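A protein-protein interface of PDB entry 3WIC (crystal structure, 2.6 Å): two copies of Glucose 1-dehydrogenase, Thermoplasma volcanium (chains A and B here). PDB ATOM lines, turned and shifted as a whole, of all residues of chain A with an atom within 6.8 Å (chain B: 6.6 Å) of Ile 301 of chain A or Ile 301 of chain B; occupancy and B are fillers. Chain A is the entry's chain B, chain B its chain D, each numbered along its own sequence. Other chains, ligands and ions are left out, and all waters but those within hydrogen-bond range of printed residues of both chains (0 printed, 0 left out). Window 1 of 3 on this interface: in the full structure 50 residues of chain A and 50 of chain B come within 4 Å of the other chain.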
ATOM      1  N   ARG A 174      -9.354   5.943 -15.355  1.00  0.00           N
ATOM      2  CA  ARG A 174      -8.966   6.524 -16.653  1.00  0.00           C
ATOM      3  C   ARG A 174      -9.561   7.906 -16.863  1.00  0.00           C
ATOM      4  O   ARG A 174      -8.964   8.761 -17.472  1.00  0.00           O
ATOM      5  CB  ARG A 174      -9.569   5.716 -17.769  1.00  0.00           C
ATOM      6  CG  ARG A 174      -8.733   4.597 -18.273  1.00  0.00           C
ATOM      7  CD  ARG A 174      -9.485   3.902 -19.401  1.00  0.00           C
ATOM      8  NE  ARG A 174      -9.383   4.620 -20.669  1.00  0.00           N
ATOM      9  CZ  ARG A 174      -9.645   4.090 -21.880  1.00  0.00           C
ATOM     10  NH1 ARG A 174     -10.078   2.836 -22.028  1.00  0.00           N
ATOM     11  NH2 ARG A 174      -9.484   4.846 -22.960  1.00  0.00           N
ATOM     12  N   ILE A 259     -21.858 -10.845 -25.777  1.00  0.00           N
ATOM     13  CA  ILE A 259     -20.932  -9.849 -25.256  1.00  0.00           C
ATOM     14  C   ILE A 259     -20.877  -8.579 -26.135  1.00  0.00           C
ATOM     15  O   ILE A 259     -21.140  -7.422 -25.650  1.00  0.00           O
ATOM     16  CB  ILE A 259     -19.527 -10.376 -25.064  1.00  0.00           C
ATOM     17  CG1 ILE A 259     -19.488 -11.423 -23.930  1.00  0.00           C
ATOM     18  CG2 ILE A 259     -18.602  -9.186 -24.791  1.00  0.00           C
ATOM     19  CD1 ILE A 259     -18.421 -12.510 -24.096  1.00  0.00           C
ATOM     20  N   PHE A 260     -20.544  -8.824 -27.400  1.00  0.00           N
ATOM     21  CA  PHE A 260     -20.257  -7.771 -28.356  1.00  0.00           C
ATOM     22  C   PHE A 260     -21.522  -7.046 -28.778  1.00  0.00           C
ATOM     23  O   PHE A 260     -21.493  -5.878 -29.107  1.00  0.00           O
ATOM     24  CB  PHE A 260     -19.481  -8.354 -29.566  1.00  0.00           C
ATOM     25  CG  PHE A 260     -18.032  -8.586 -29.263  1.00  0.00           C
ATOM     26  CD1 PHE A 260     -17.144  -7.513 -29.230  1.00  0.00           C
ATOM     27  CD2 PHE A 260     -17.562  -9.842 -28.929  1.00  0.00           C
ATOM     28  CE1 PHE A 260     -15.819  -7.702 -28.904  1.00  0.00           C
ATOM     29  CE2 PHE A 260     -16.227 -10.028 -28.596  1.00  0.00           C
ATOM     30  CZ  PHE A 260     -15.361  -8.951 -28.587  1.00  0.00           C
ATOM     31  N   VAL A 263     -21.734  -4.950 -25.974  1.00  0.00           N
ATOM     32  CA  VAL A 263     -20.616  -3.997 -26.056  1.00  0.00           C
ATOM     33  C   VAL A 263     -21.035  -2.733 -26.851  1.00  0.00           C
ATOM     34  O   VAL A 263     -20.709  -1.602 -26.484  1.00  0.00           O
ATOM     35  CB  VAL A 263     -19.330  -4.670 -26.614  1.00  0.00           C
ATOM     36  CG1 VAL A 263     -18.289  -3.643 -27.002  1.00  0.00           C
ATOM     37  CG2 VAL A 263     -18.707  -5.605 -25.592  1.00  0.00           C
ATOM     38  N   GLY A 270     -17.146   3.676 -20.848  1.00  0.00           N
ATOM     39  CA  GLY A 270     -17.764   2.446 -20.338  1.00  0.00           C
ATOM     40  C   GLY A 270     -16.715   1.417 -19.987  1.00  0.00           C
ATOM     41  O   GLY A 270     -15.579   1.503 -20.474  1.00  0.00           O
ATOM     42  N   VAL A 271     -17.063   0.490 -19.086  1.00  0.00           N
ATOM     43  CA  VAL A 271     -16.177  -0.628 -18.723  1.00  0.00           C
ATOM     44  C   VAL A 271     -16.942  -1.915 -18.861  1.00  0.00           C
ATOM     45  O   VAL A 271     -18.060  -1.984 -18.474  1.00  0.00           O
ATOM     46  CB  VAL A 271     -15.631  -0.563 -17.260  1.00  0.00           C
ATOM     47  CG1 VAL A 271     -14.816  -1.813 -16.925  1.00  0.00           C
ATOM     48  CG2 VAL A 271     -14.803   0.721 -17.034  1.00  0.00           C
ATOM     49  N   VAL A 272     -16.303  -2.936 -19.405  1.00  0.00           N
ATOM     50  CA  VAL A 272     -16.894  -4.194 -19.627  1.00  0.00           C
ATOM     51  C   VAL A 272     -15.958  -5.075 -18.896  1.00  0.00           C
ATOM     52  O   VAL A 272     -14.756  -4.873 -19.013  1.00  0.00           O
ATOM     53  CB  VAL A 272     -16.871  -4.540 -21.116  1.00  0.00           C
ATOM     54  CG1 VAL A 272     -17.281  -5.985 -21.382  1.00  0.00           C
ATOM     55  CG2 VAL A 272     -17.737  -3.552 -21.891  1.00  0.00           C
ATOM     56  N   ILE A 273     -16.511  -6.011 -18.125  1.00  0.00           N
ATOM     57  CA  ILE A 273     -15.785  -7.016 -17.431  1.00  0.00           C
ATOM     58  C   ILE A 273     -16.145  -8.354 -18.062  1.00  0.00           C
ATOM     59  O   ILE A 273     -17.329  -8.759 -18.155  1.00  0.00           O
ATOM     60  CB  ILE A 273     -16.171  -7.099 -15.941  1.00  0.00           C
ATOM     61  CG1 ILE A 273     -15.876  -5.788 -15.174  1.00  0.00           C
ATOM     62  CG2 ILE A 273     -15.441  -8.241 -15.275  1.00  0.00           C
ATOM     63  CD1 ILE A 273     -14.455  -5.337 -15.181  1.00  0.00           C
ATOM     64  N   LEU A 274     -15.120  -9.093 -18.422  1.00  0.00           N
ATOM     65  CA  LEU A 274     -15.295 -10.423 -18.922  1.00  0.00           C
ATOM     66  C   LEU A 274     -14.920 -11.352 -17.794  1.00  0.00           C
ATOM     67  O   LEU A 274     -13.864 -11.259 -17.287  1.00  0.00           O
ATOM     68  CB  LEU A 274     -14.407 -10.648 -20.170  1.00  0.00           C
ATOM     69  CG  LEU A 274     -14.523  -9.770 -21.397  1.00  0.00           C
ATOM     70  CD1 LEU A 274     -13.556 -10.239 -22.437  1.00  0.00           C
ATOM     71  CD2 LEU A 274     -15.921  -9.736 -21.954  1.00  0.00           C
ATOM     72  N   ILE A 294     -15.436   0.906 -29.859  1.00  0.00           N
ATOM     73  CA  ILE A 294     -14.722   0.773 -28.621  1.00  0.00           C
ATOM     74  C   ILE A 294     -13.731   1.894 -28.433  1.00  0.00           C
ATOM     75  O   ILE A 294     -13.671   2.542 -27.361  1.00  0.00           O
ATOM     76  CB  ILE A 294     -14.026  -0.562 -28.590  1.00  0.00           C
ATOM     77  CG1 ILE A 294     -15.086  -1.636 -28.456  1.00  0.00           C
ATOM     78  CG2 ILE A 294     -13.072  -0.629 -27.400  1.00  0.00           C
ATOM     79  CD1 ILE A 294     -14.606  -3.050 -28.775  1.00  0.00           C
ATOM     80  N   ILE A 299     -13.469   2.995 -24.235  1.00  0.00           N
ATOM     81  CA  ILE A 299     -14.023   1.928 -23.455  1.00  0.00           C
ATOM     82  C   ILE A 299     -12.919   0.982 -23.011  1.00  0.00           C
ATOM     83  O   ILE A 299     -11.925   0.869 -23.682  1.00  0.00           O
ATOM     84  CB  ILE A 299     -15.055   1.170 -24.320  1.00  0.00           C
ATOM     85  CG1 ILE A 299     -16.328   2.033 -24.461  1.00  0.00           C
ATOM     86  CG2 ILE A 299     -15.358  -0.236 -23.770  1.00  0.00           C
ATOM     87  CD1 ILE A 299     -17.279   1.569 -25.547  1.00  0.00           C
ATOM     88  N   THR A 300     -13.095   0.261 -21.911  1.00  0.00           N
ATOM     89  CA  THR A 300     -12.093  -0.714 -21.417  1.00  0.00           C
ATOM     90  C   THR A 300     -12.738  -2.091 -21.266  1.00  0.00           C
ATOM     91  O   THR A 300     -13.828  -2.219 -20.731  1.00  0.00           O
ATOM     92  CB  THR A 300     -11.533  -0.251 -20.068  1.00  0.00           C
ATOM     93  OG1 THR A 300     -11.104   1.122 -20.163  1.00  0.00           O
ATOM     94  CG2 THR A 300     -10.418  -1.107 -19.577  1.00  0.00           C
ATOM     95  N   ILE A 301     -12.101  -3.114 -21.811  1.00  0.00           N
ATOM     96  CA  ILE A 301     -12.597  -4.475 -21.690  1.00  0.00           C
ATOM     97  C   ILE A 301     -11.579  -5.169 -20.842  1.00  0.00           C
ATOM     98  O   ILE A 301     -10.434  -5.353 -21.255  1.00  0.00           O
ATOM     99  CB  ILE A 301     -12.751  -5.217 -23.052  1.00  0.00           C
ATOM    100  CG1 ILE A 301     -13.646  -4.399 -23.975  1.00  0.00           C
ATOM    101  CG2 ILE A 301     -13.343  -6.618 -22.860  1.00  0.00           C
ATOM    102  CD1 ILE A 301     -13.887  -5.066 -25.301  1.00  0.00           C
ATOM    103  N   ALA A 302     -11.970  -5.502 -19.628  1.00  0.00           N
ATOM    104  CA  ALA A 302     -11.039  -6.083 -18.694  1.00  0.00           C
ATOM    105  C   ALA A 302     -11.468  -7.499 -18.420  1.00  0.00           C
ATOM    106  O   ALA A 302     -12.561  -7.727 -17.907  1.00  0.00           O
ATOM    107  CB  ALA A 302     -10.991  -5.261 -17.402  1.00  0.00           C
ATOM    108  N   GLY A 303     -10.622  -8.450 -18.805  1.00  0.00           N
ATOM    109  CA  GLY A 303     -10.805  -9.842 -18.367  1.00  0.00           C
ATOM    110  C   GLY A 303     -10.411  -9.906 -16.924  1.00  0.00           C
ATOM    111  O   GLY A 303      -9.422  -9.289 -16.561  1.00  0.00           O
ATOM    112  N   ARG B 174      -3.514  -2.558 -12.046  1.00  0.00           N
ATOM    113  CA  ARG B 174      -4.308  -3.671 -11.584  1.00  0.00           C
ATOM    114  C   ARG B 174      -3.492  -4.809 -11.031  1.00  0.00           C
ATOM    115  O   ARG B 174      -3.983  -5.594 -10.262  1.00  0.00           O
ATOM    116  CB  ARG B 174      -5.314  -4.115 -12.637  1.00  0.00           C
ATOM    117  CG  ARG B 174      -4.780  -4.702 -13.901  1.00  0.00           C
ATOM    118  CD  ARG B 174      -5.973  -5.184 -14.739  1.00  0.00           C
ATOM    119  NE  ARG B 174      -6.503  -6.442 -14.199  1.00  0.00           N
ATOM    120  CZ  ARG B 174      -7.295  -7.278 -14.851  1.00  0.00           C
ATOM    121  NH1 ARG B 174      -7.675  -7.022 -16.089  1.00  0.00           N
ATOM    122  NH2 ARG B 174      -7.707  -8.375 -14.246  1.00  0.00           N
ATOM    123  N   ILE B 259      -5.687  -7.791 -34.806  1.00  0.00           N
ATOM    124  CA  ILE B 259      -5.813  -7.488 -33.373  1.00  0.00           C
ATOM    125  C   ILE B 259      -5.857  -8.749 -32.533  1.00  0.00           C
ATOM    126  O   ILE B 259      -5.044  -8.906 -31.608  1.00  0.00           O
ATOM    127  CB  ILE B 259      -7.063  -6.661 -33.080  1.00  0.00           C
ATOM    128  CG1 ILE B 259      -6.858  -5.208 -33.558  1.00  0.00           C
ATOM    129  CG2 ILE B 259      -7.349  -6.676 -31.598  1.00  0.00           C
ATOM    130  CD1 ILE B 259      -8.124  -4.402 -33.744  1.00  0.00           C
ATOM    131  N   PHE B 260      -6.775  -9.660 -32.879  1.00  0.00           N
ATOM    132  CA  PHE B 260      -7.004 -10.905 -32.113  1.00  0.00           C
ATOM    133  C   PHE B 260      -5.983 -12.014 -32.331  1.00  0.00           C
ATOM    134  O   PHE B 260      -5.743 -12.822 -31.455  1.00  0.00           O
ATOM    135  CB  PHE B 260      -8.429 -11.433 -32.358  1.00  0.00           C
ATOM    136  CG  PHE B 260      -9.469 -10.667 -31.601  1.00  0.00           C
ATOM    137  CD1 PHE B 260      -9.644 -10.868 -30.263  1.00  0.00           C
ATOM    138  CD2 PHE B 260     -10.231  -9.702 -32.226  1.00  0.00           C
ATOM    139  CE1 PHE B 260     -10.587 -10.127 -29.554  1.00  0.00           C
ATOM    140  CE2 PHE B 260     -11.179  -8.961 -31.524  1.00  0.00           C
ATOM    141  CZ  PHE B 260     -11.359  -9.176 -30.189  1.00  0.00           C
ATOM    142  N   VAL B 263      -3.476 -10.675 -29.832  1.00  0.00           N
ATOM    143  CA  VAL B 263      -4.007 -10.850 -28.474  1.00  0.00           C
ATOM    144  C   VAL B 263      -3.629 -12.233 -27.925  1.00  0.00           C
ATOM    145  O   VAL B 263      -3.341 -12.383 -26.746  1.00  0.00           O
ATOM    146  CB  VAL B 263      -5.547 -10.651 -28.459  1.00  0.00           C
ATOM    147  CG1 VAL B 263      -6.215 -11.451 -27.361  1.00  0.00           C
ATOM    148  CG2 VAL B 263      -5.915  -9.176 -28.380  1.00  0.00           C
ATOM    149  N   GLY B 270      -1.259  -8.842 -19.352  1.00  0.00           N
ATOM    150  CA  GLY B 270      -0.935  -8.052 -20.557  1.00  0.00           C
ATOM    151  C   GLY B 270      -1.969  -6.953 -20.769  1.00  0.00           C
ATOM    152  O   GLY B 270      -3.056  -7.075 -20.302  1.00  0.00           O
ATOM    153  N   VAL B 271      -1.575  -5.884 -21.434  1.00  0.00           N
ATOM    154  CA  VAL B 271      -2.432  -4.741 -21.749  1.00  0.00           C
ATOM    155  C   VAL B 271      -2.423  -4.590 -23.274  1.00  0.00           C
ATOM    156  O   VAL B 271      -1.403  -4.686 -23.845  1.00  0.00           O
ATOM    157  CB  VAL B 271      -1.894  -3.445 -21.143  1.00  0.00           C
ATOM    158  CG1 VAL B 271      -2.665  -2.256 -21.682  1.00  0.00           C
ATOM    159  CG2 VAL B 271      -1.979  -3.486 -19.631  1.00  0.00           C
ATOM    160  N   VAL B 272      -3.572  -4.390 -23.910  1.00  0.00           N
ATOM    161  CA  VAL B 272      -3.698  -4.210 -25.350  1.00  0.00           C
ATOM    162  C   VAL B 272      -4.306  -2.833 -25.569  1.00  0.00           C
ATOM    163  O   VAL B 272      -5.368  -2.541 -25.046  1.00  0.00           O
ATOM    164  CB  VAL B 272      -4.667  -5.267 -25.965  1.00  0.00           C
ATOM    165  CG1 VAL B 272      -5.030  -4.950 -27.399  1.00  0.00           C
ATOM    166  CG2 VAL B 272      -4.102  -6.664 -25.848  1.00  0.00           C
ATOM    167  N   ILE B 273      -3.628  -1.966 -26.304  1.00  0.00           N
ATOM    168  CA  ILE B 273      -4.193  -0.646 -26.625  1.00  0.00           C
ATOM    169  C   ILE B 273      -4.761  -0.647 -28.036  1.00  0.00           C
ATOM    170  O   ILE B 273      -4.072  -0.940 -28.982  1.00  0.00           O
ATOM    171  CB  ILE B 273      -3.107   0.400 -26.608  1.00  0.00           C
ATOM    172  CG1 ILE B 273      -2.395   0.349 -25.289  1.00  0.00           C
ATOM    173  CG2 ILE B 273      -3.679   1.780 -26.910  1.00  0.00           C
ATOM    174  CD1 ILE B 273      -3.256   0.756 -24.126  1.00  0.00           C
ATOM    175  N   LEU B 274      -6.015  -0.301 -28.185  1.00  0.00           N
ATOM    176  CA  LEU B 274      -6.639  -0.244 -29.468  1.00  0.00           C
ATOM    177  C   LEU B 274      -6.663   1.206 -29.810  1.00  0.00           C
ATOM    178  O   LEU B 274      -7.162   1.993 -29.075  1.00  0.00           O
ATOM    179  CB  LEU B 274      -8.052  -0.812 -29.410  1.00  0.00           C
ATOM    180  CG  LEU B 274      -8.303  -2.252 -29.040  1.00  0.00           C
ATOM    181  CD1 LEU B 274      -9.781  -2.393 -28.871  1.00  0.00           C
ATOM    182  CD2 LEU B 274      -7.844  -3.219 -30.093  1.00  0.00           C
ATOM    183  N   ILE B 294      -8.411 -14.305 -22.813  1.00  0.00           N
ATOM    184  CA  ILE B 294      -8.394 -13.008 -22.234  1.00  0.00           C
ATOM    185  C   ILE B 294      -8.747 -13.076 -20.752  1.00  0.00           C
ATOM    186  O   ILE B 294      -8.102 -12.421 -19.932  1.00  0.00           O
ATOM    187  CB  ILE B 294      -9.361 -12.076 -22.971  1.00  0.00           C
ATOM    188  CG1 ILE B 294      -8.861 -11.836 -24.399  1.00  0.00           C
ATOM    189  CG2 ILE B 294      -9.535 -10.785 -22.189  1.00  0.00           C
ATOM    190  CD1 ILE B 294      -9.892 -11.166 -25.305  1.00  0.00           C
ATOM    191  N   ILE B 299      -6.180 -10.086 -18.838  1.00  0.00           N
ATOM    192  CA  ILE B 299      -5.718  -9.157 -19.854  1.00  0.00           C
ATOM    193  C   ILE B 299      -6.677  -7.995 -19.940  1.00  0.00           C
ATOM    194  O   ILE B 299      -7.865  -8.144 -19.720  1.00  0.00           O
ATOM    195  CB  ILE B 299      -5.579  -9.846 -21.218  1.00  0.00           C
ATOM    196  CG1 ILE B 299      -4.380 -10.781 -21.160  1.00  0.00           C
ATOM    197  CG2 ILE B 299      -5.384  -8.824 -22.332  1.00  0.00           C
ATOM    198  CD1 ILE B 299      -4.225 -11.719 -22.362  1.00  0.00           C
ATOM    199  N   THR B 300      -6.155  -6.825 -20.262  1.00  0.00           N
ATOM    200  CA  THR B 300      -6.986  -5.629 -20.387  1.00  0.00           C
ATOM    201  C   THR B 300      -6.897  -5.085 -21.790  1.00  0.00           C
ATOM    202  O   THR B 300      -5.811  -4.837 -22.290  1.00  0.00           O
ATOM    203  CB  THR B 300      -6.554  -4.505 -19.437  1.00  0.00           C
ATOM    204  OG1 THR B 300      -6.343  -5.030 -18.147  1.00  0.00           O
ATOM    205  CG2 THR B 300      -7.580  -3.473 -19.332  1.00  0.00           C
ATOM    206  N   ILE B 301      -8.053  -4.856 -22.391  1.00  0.00           N
ATOM    207  CA  ILE B 301      -8.123  -4.338 -23.729  1.00  0.00           C
ATOM    208  C   ILE B 301      -8.805  -2.977 -23.630  1.00  0.00           C
ATOM    209  O   ILE B 301      -9.987  -2.908 -23.293  1.00  0.00           O
ATOM    210  CB  ILE B 301      -8.902  -5.288 -24.648  1.00  0.00           C
ATOM    211  CG1 ILE B 301      -8.179  -6.613 -24.828  1.00  0.00           C
ATOM    212  CG2 ILE B 301      -9.112  -4.648 -26.016  1.00  0.00           C
ATOM    213  CD1 ILE B 301      -9.100  -7.651 -25.414  1.00  0.00           C
ATOM    214  N   ALA B 302      -8.039  -1.913 -23.888  1.00  0.00           N
ATOM    215  CA  ALA B 302      -8.534  -0.587 -23.793  1.00  0.00           C
ATOM    216  C   ALA B 302      -8.432   0.160 -25.119  1.00  0.00           C
ATOM    217  O   ALA B 302      -7.407   0.180 -25.710  1.00  0.00           O
ATOM    218  CB  ALA B 302      -7.791   0.169 -22.706  1.00  0.00           C
ATOM    219  N   GLY B 303      -9.496   0.822 -25.545  1.00  0.00           N
ATOM    220  CA  GLY B 303      -9.436   1.629 -26.714  1.00  0.00           C
ATOM    221  C   GLY B 303      -9.182   3.054 -26.299  1.00  0.00           C
ATOM    222  O   GLY B 303      -9.663   3.461 -25.292  1.00  0.00           O
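Ile 299 of chain A touches Ala 302 of chain B, and with the chains exchanged Ala 302 of chain A touches Ile 299 of chain B.
Ile 299 of chain A touches Gly 303 of chain B, and with the chains exchanged Gly 303 of chain A touches Ile 299 of chain B.
Thr 300 of chain A touches Ile 301 of chain B, and with the chains exchanged Ile 301 of chain A touches Thr 300 of chain B.
Ile 301 of chain A touches its own counterpart, Ile 301 of chain B.
NH2 of Arg 174 of chain A lies within hydrogen-bond range of O of Gly 303 of chain B, at 2.7 Å.
The backbone carbonyl oxygen (O) of Ile 299 of chain A is in hydrogen-bond range of the backbone NH (N) of Gly 303 of chain B (3.1 Å).
O of Gly 303 of chain A is in hydrogen-bond range of NH1 of Arg 174 of chain B, at 2.9 Å.
O of Ile 301 of chain B is in hydrogen-bond range of N of Ile 301 of chain A, 2.6 Å away.
N of Gly 303 of chain A is in hydrogen-bond range of O of Ile 299 of chain B (2.9 Å).
Val 272 of chain A touches none of the printed residues of chain B.
Ile 301 of chain A touches just these residues of chain B: Thr 300 (3.6 Å) and Ile 301 (2.6 Å).
Of the printed residues of chain B, Gly 303 of chain A touches Arg 174 (2.9 Å) and Ile 299 (2.9 Å).
Printed residues of chain A within 4 Å of Ile 299 of chain B: Ala 302 (3.9 Å) and Gly 303 (2.9 Å).
Of the printed residues of chain A, Thr 300 of chain B touches Thr 300 and Ile 301.
Ile 301 of chain B touches just these residues of chain A: Thr 300 (3.5 Å) and Ile 301 (2.6 Å).
The nearest residue of chain B that does not touch Ile 301 of chain A is Ile 299 of chain B (4.1 Å).
The nearest residue of chain A that does not touch Ile 301 of chain B is Ile 299 of chain A (4.3 Å).
The nearest printed residue of chain A that does not touch Thr 300 of chain B is Ala 302 of chain A (4.3 Å).
Of the 15 printed residues of chain A, 6 touch a printed residue of chain B.
Hydrophobic or aromatic side chains of chain A within 4 Å of the printed part of chain B: Ile 301 and Ala 302.
Printed residues of chain B that touch a printed residue of chain A: Arg 174, Ile 299, Thr 300, Ile 301, Ala 302 and Gly 303.
Hydrophobic or aromatic side chains of chain B within 4 Å of the printed part of chain A: Ile 301 and Ala 302.
Among the printed residues, 12 pairs touch across the chains.
Among the printed residues, no Asp or Glu carboxylate lies within 4 Å of a Lys or Arg side-chain nitrogen of the other chain.
Among the printed residues, pairs that only touch across the chains: Arg 174 of chain A with Ala 302 of chain B, Ile 299 of chain A with Ala 302 of chain B, Thr 300 of chain A with Thr 300 of chain B, Thr 300 of chain A with Ile 301 of chain B, Ile 301 of chain A with Thr 300 of chain B, Ala 302 of chain A with Arg 174 of chain B and Ala 302 of chain A with Ile 299 of chain B.
N of Ala 302 of chain A is in hydrogen-bond range of O of Val 272 of chain A, 2.9 Å away.
The backbone carbonyl oxygen of Ile 294 of chain A sits at hydrogen-bond distance from the backbone NH of Ile 299 of chain A (3.2 Å).
NH1 of Arg 174 of chain B lies within hydrogen-bond range of OG1 of Thr 300 of chain B (3.2 Å).
N of Val 272 of chain A lies within hydrogen-bond range of O of Thr 300 of chain A.
The backbone carbonyl oxygen (O) of Gly 270 of chain B sits at hydrogen-bond distance from the backbone NH (N) of Thr 300 of chain B, at 3.1 Å.
The backbone carbonyl oxygen (O) of Ile 294 of chain B is in hydrogen-bond range of the backbone NH (N) of Ile 299 of chain B.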
